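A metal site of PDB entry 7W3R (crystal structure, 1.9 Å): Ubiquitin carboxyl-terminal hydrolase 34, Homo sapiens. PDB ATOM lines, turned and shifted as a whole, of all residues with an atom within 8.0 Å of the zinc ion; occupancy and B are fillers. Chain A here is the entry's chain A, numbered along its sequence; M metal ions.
The zinc ion is bound by ND1 of His 132 (2.1 Å), SG of Cys 177 (2.1 Å), SG of Cys 174 (2.3 Å) and SG of Cys 130 (2.3 Å).
Within 4 Å of the zinc ion: Cys 130, His 132, Cys 174 and Cys 177.
The nearest printed residue that does not touch the zinc ion is His 176 (4.4 Å).
The backbone NH of His 176 sits close to the side-chain sulfur of Cys 174, at 3.4 Å.
N of Ser 127 lies within hydrogen-bond range of O of His 132 (3.5 Å).
N of Cys 174 sits at hydrogen-bond distance from O of Lys 179, 3.1 Å away.
N of Cys 130 is in hydrogen-bond range of OG of Ser 127 (2.8 Å).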
ATOM      1  N   SER A 127     -27.604   1.415  17.250  1.00  0.00           N
ATOM      2  CA  SER A 127     -27.238   0.531  18.351  1.00  0.00           C
ATOM      3  C   SER A 127     -27.415  -0.925  17.945  1.00  0.00           C
ATOM      4  O   SER A 127     -28.365  -1.277  17.230  1.00  0.00           O
ATOM      5  CB  SER A 127     -28.056   0.857  19.611  1.00  0.00           C
ATOM      6  OG  SER A 127     -28.050  -0.161  20.608  1.00  0.00           O
ATOM      7  N   ASP A 129     -27.399  -3.189  20.491  1.00  0.00           N
ATOM      8  CA  ASP A 129     -27.842  -3.827  21.709  1.00  0.00           C
ATOM      9  C   ASP A 129     -29.083  -3.156  22.288  1.00  0.00           C
ATOM     10  O   ASP A 129     -29.442  -3.442  23.429  1.00  0.00           O
ATOM     11  CB  ASP A 129     -26.720  -3.848  22.760  1.00  0.00           C
ATOM     12  CG  ASP A 129     -25.488  -4.591  22.259  1.00  0.00           C
ATOM     13  OD1 ASP A 129     -25.627  -5.735  21.803  1.00  0.00           O
ATOM     14  OD2 ASP A 129     -24.381  -4.035  22.344  1.00  0.00           O
ATOM     15  N   CYS A 130     -29.718  -2.263  21.536  1.00  0.00           N
ATOM     16  CA  CYS A 130     -31.041  -1.758  21.845  1.00  0.00           C
ATOM     17  C   CYS A 130     -31.690  -1.336  20.539  1.00  0.00           C
ATOM     18  O   CYS A 130     -31.073  -1.398  19.473  1.00  0.00           O
ATOM     19  CB  CYS A 130     -31.009  -0.585  22.851  1.00  0.00           C
ATOM     20  SG  CYS A 130     -30.228   0.899  22.207  1.00  0.00           S
ATOM     21  N   GLU A 131     -32.935  -0.876  20.630  1.00  0.00           N
ATOM     22  CA  GLU A 131     -33.668  -0.487  19.434  1.00  0.00           C
ATOM     23  C   GLU A 131     -33.390   0.936  18.970  1.00  0.00           C
ATOM     24  O   GLU A 131     -33.817   1.318  17.884  1.00  0.00           O
ATOM     25  CB  GLU A 131     -35.167  -0.664  19.678  1.00  0.00           C
ATOM     26  CG  GLU A 131     -35.687   0.127  20.878  1.00  0.00           C
ATOM     27  CD  GLU A 131     -35.647  -0.665  22.173  1.00  0.00           C
ATOM     28  OE1 GLU A 131     -36.672  -0.663  22.899  1.00  0.00           O
ATOM     29  OE2 GLU A 131     -34.597  -1.274  22.483  1.00  0.00           O
ATOM     30  N   HIS A 132     -32.668   1.734  19.751  1.00  0.00           N
ATOM     31  CA  HIS A 132     -32.649   3.169  19.492  1.00  0.00           C
ATOM     32  C   HIS A 132     -31.638   3.563  18.439  1.00  0.00           C
ATOM     33  O   HIS A 132     -30.586   2.932  18.270  1.00  0.00           O
ATOM     34  CB  HIS A 132     -32.386   3.931  20.789  1.00  0.00           C
ATOM     35  CG  HIS A 132     -33.368   3.607  21.854  1.00  0.00           C
ATOM     36  ND1 HIS A 132     -33.051   2.862  22.971  1.00  0.00           N
ATOM     37  CD2 HIS A 132     -34.695   3.875  21.939  1.00  0.00           C
ATOM     38  CE1 HIS A 132     -34.136   2.703  23.710  1.00  0.00           C
ATOM     39  NE2 HIS A 132     -35.146   3.308  23.102  1.00  0.00           N
ATOM     40  N   VAL A 133     -31.979   4.620  17.715  1.00  0.00           N
ATOM     41  CA  VAL A 133     -31.100   5.201  16.717  1.00  0.00           C
ATOM     42  C   VAL A 133     -30.969   6.688  17.051  1.00  0.00           C
ATOM     43  O   VAL A 133     -31.838   7.284  17.687  1.00  0.00           O
ATOM     44  CB  VAL A 133     -31.620   4.988  15.277  1.00  0.00           C
ATOM     45  CG1 VAL A 133     -31.683   3.492  14.970  1.00  0.00           C
ATOM     46  CG2 VAL A 133     -32.992   5.640  15.124  1.00  0.00           C
ATOM     47  N   TYR A 172     -20.679   2.892  23.070  1.00  0.00           N
ATOM     48  CA  TYR A 172     -21.597   4.019  23.015  1.00  0.00           C
ATOM     49  C   TYR A 172     -22.547   3.983  24.201  1.00  0.00           C
ATOM     50  O   TYR A 172     -22.927   2.909  24.698  1.00  0.00           O
ATOM     51  CB  TYR A 172     -22.401   3.969  21.714  1.00  0.00           C
ATOM     52  CG  TYR A 172     -23.350   5.109  21.435  1.00  0.00           C
ATOM     53  CD1 TYR A 172     -22.890   6.326  20.915  1.00  0.00           C
ATOM     54  CD2 TYR A 172     -24.728   4.965  21.620  1.00  0.00           C
ATOM     55  CE1 TYR A 172     -23.766   7.367  20.625  1.00  0.00           C
ATOM     56  CE2 TYR A 172     -25.612   6.006  21.324  1.00  0.00           C
ATOM     57  CZ  TYR A 172     -25.127   7.203  20.837  1.00  0.00           C
ATOM     58  OH  TYR A 172     -25.989   8.235  20.545  1.00  0.00           O
ATOM     59  N   THR A 173     -22.935   5.160  24.669  1.00  0.00           N
ATOM     60  CA  THR A 173     -24.014   5.246  25.647  1.00  0.00           C
ATOM     61  C   THR A 173     -25.238   5.770  24.923  1.00  0.00           C
ATOM     62  O   THR A 173     -25.221   6.851  24.324  1.00  0.00           O
ATOM     63  CB  THR A 173     -23.658   6.111  26.854  1.00  0.00           C
ATOM     64  OG1 THR A 173     -23.542   7.490  26.453  1.00  0.00           O
ATOM     65  CG2 THR A 173     -22.349   5.641  27.467  1.00  0.00           C
ATOM     66  N   CYS A 174     -26.263   4.935  24.881  1.00  0.00           N
ATOM     67  CA  CYS A 174     -27.530   5.315  24.296  1.00  0.00           C
ATOM     68  C   CYS A 174     -28.184   6.320  25.211  1.00  0.00           C
ATOM     69  O   CYS A 174     -28.265   6.088  26.416  1.00  0.00           O
ATOM     70  CB  CYS A 174     -28.417   4.084  24.159  1.00  0.00           C
ATOM     71  SG  CYS A 174     -30.008   4.471  23.503  1.00  0.00           S
ATOM     72  N   SER A 175     -28.619   7.453  24.657  1.00  0.00           N
ATOM     73  CA  SER A 175     -29.240   8.469  25.496  1.00  0.00           C
ATOM     74  C   SER A 175     -30.656   8.080  25.911  1.00  0.00           C
ATOM     75  O   SER A 175     -31.135   8.555  26.944  1.00  0.00           O
ATOM     76  CB  SER A 175     -29.264   9.811  24.785  1.00  0.00           C
ATOM     77  OG  SER A 175     -27.979  10.432  24.769  1.00  0.00           O
ATOM     78  N   HIS A 176     -31.295   7.193  25.153  1.00  0.00           N
ATOM     79  CA  HIS A 176     -32.678   6.787  25.428  1.00  0.00           C
ATOM     80  C   HIS A 176     -32.780   5.805  26.596  1.00  0.00           C
ATOM     81  O   HIS A 176     -33.560   6.017  27.529  1.00  0.00           O
ATOM     82  CB  HIS A 176     -33.291   6.209  24.159  1.00  0.00           C
ATOM     83  CG  HIS A 176     -33.586   7.263  23.130  1.00  0.00           C
ATOM     84  ND1 HIS A 176     -34.721   8.034  23.176  1.00  0.00           N
ATOM     85  CD2 HIS A 176     -32.869   7.712  22.080  1.00  0.00           C
ATOM     86  CE1 HIS A 176     -34.704   8.902  22.167  1.00  0.00           C
ATOM     87  NE2 HIS A 176     -33.583   8.721  21.497  1.00  0.00           N
ATOM     88  N   CYS A 177     -32.036   4.706  26.568  1.00  0.00           N
ATOM     89  CA  CYS A 177     -32.145   3.775  27.680  1.00  0.00           C
ATOM     90  C   CYS A 177     -30.977   3.896  28.670  1.00  0.00           C
ATOM     91  O   CYS A 177     -30.973   3.228  29.701  1.00  0.00           O
ATOM     92  CB  CYS A 177     -32.296   2.352  27.158  1.00  0.00           C
ATOM     93  SG  CYS A 177     -31.242   1.922  25.772  1.00  0.00           S
ATOM     94  N   GLY A 178     -30.035   4.795  28.411  1.00  0.00           N
ATOM     95  CA  GLY A 178     -28.966   5.045  29.366  1.00  0.00           C
ATOM     96  C   GLY A 178     -27.965   3.918  29.510  1.00  0.00           C
ATOM     97  O   GLY A 178     -27.078   3.997  30.358  1.00  0.00           O
ATOM     98  N   LYS A 179     -28.077   2.881  28.675  1.00  0.00           N
ATOM     99  CA  LYS A 179     -27.235   1.692  28.732  1.00  0.00           C
ATOM    100  C   LYS A 179     -25.964   1.896  27.898  1.00  0.00           C
ATOM    101  O   LYS A 179     -25.908   2.713  26.969  1.00  0.00           O
ATOM    102  CB  LYS A 179     -28.025   0.489  28.203  1.00  0.00           C
ATOM    103  CG  LYS A 179     -27.460  -0.869  28.572  1.00  0.00           C
ATOM    104  CD  LYS A 179     -28.108  -1.975  27.727  1.00  0.00           C
ATOM    105  CE  LYS A 179     -27.072  -3.021  27.269  1.00  0.00           C
ATOM    106  NZ  LYS A 179     -26.297  -3.569  28.429  1.00  0.00           N
ATOM    107  N   LYS A 180     -24.927   1.156  28.257  1.00  0.00           N
ATOM    108  CA  LYS A 180     -23.769   1.049  27.391  1.00  0.00           C
ATOM    109  C   LYS A 180     -24.058  -0.018  26.342  1.00  0.00           C
ATOM    110  O   LYS A 180     -24.544  -1.112  26.682  1.00  0.00           O
ATOM    111  CB  LYS A 180     -22.511   0.714  28.184  1.00  0.00           C
ATOM    112  CG  LYS A 180     -21.912   1.912  28.894  1.00  0.00           C
ATOM    113  CD  LYS A 180     -22.416   2.009  30.338  1.00  0.00           C
ATOM    114  CE  LYS A 180     -21.548   2.948  31.158  1.00  0.00           C
ATOM    115  NZ  LYS A 180     -21.048   4.101  30.340  1.00  0.00           N
ATOM    116  N   VAL A 181     -23.808   0.318  25.081  1.00  0.00           N
ATOM    117  CA  VAL A 181     -24.184  -0.509  23.948  1.00  0.00           C
ATOM    118  C   VAL A 181     -23.090  -0.463  22.885  1.00  0.00           C
ATOM    119  O   VAL A 181     -22.467   0.580  22.663  1.00  0.00           O
ATOM    120  CB  VAL A 181     -25.517  -0.078  23.302  1.00  0.00           C
ATOM    121  CG1 VAL A 181     -26.651  -0.034  24.349  1.00  0.00           C
ATOM    122  CG2 VAL A 181     -25.383   1.277  22.599  1.00  0.00           C
HETATM  123 ZN    ZN M   1     -31.080   2.470  23.705  1.00  0.00          ZN
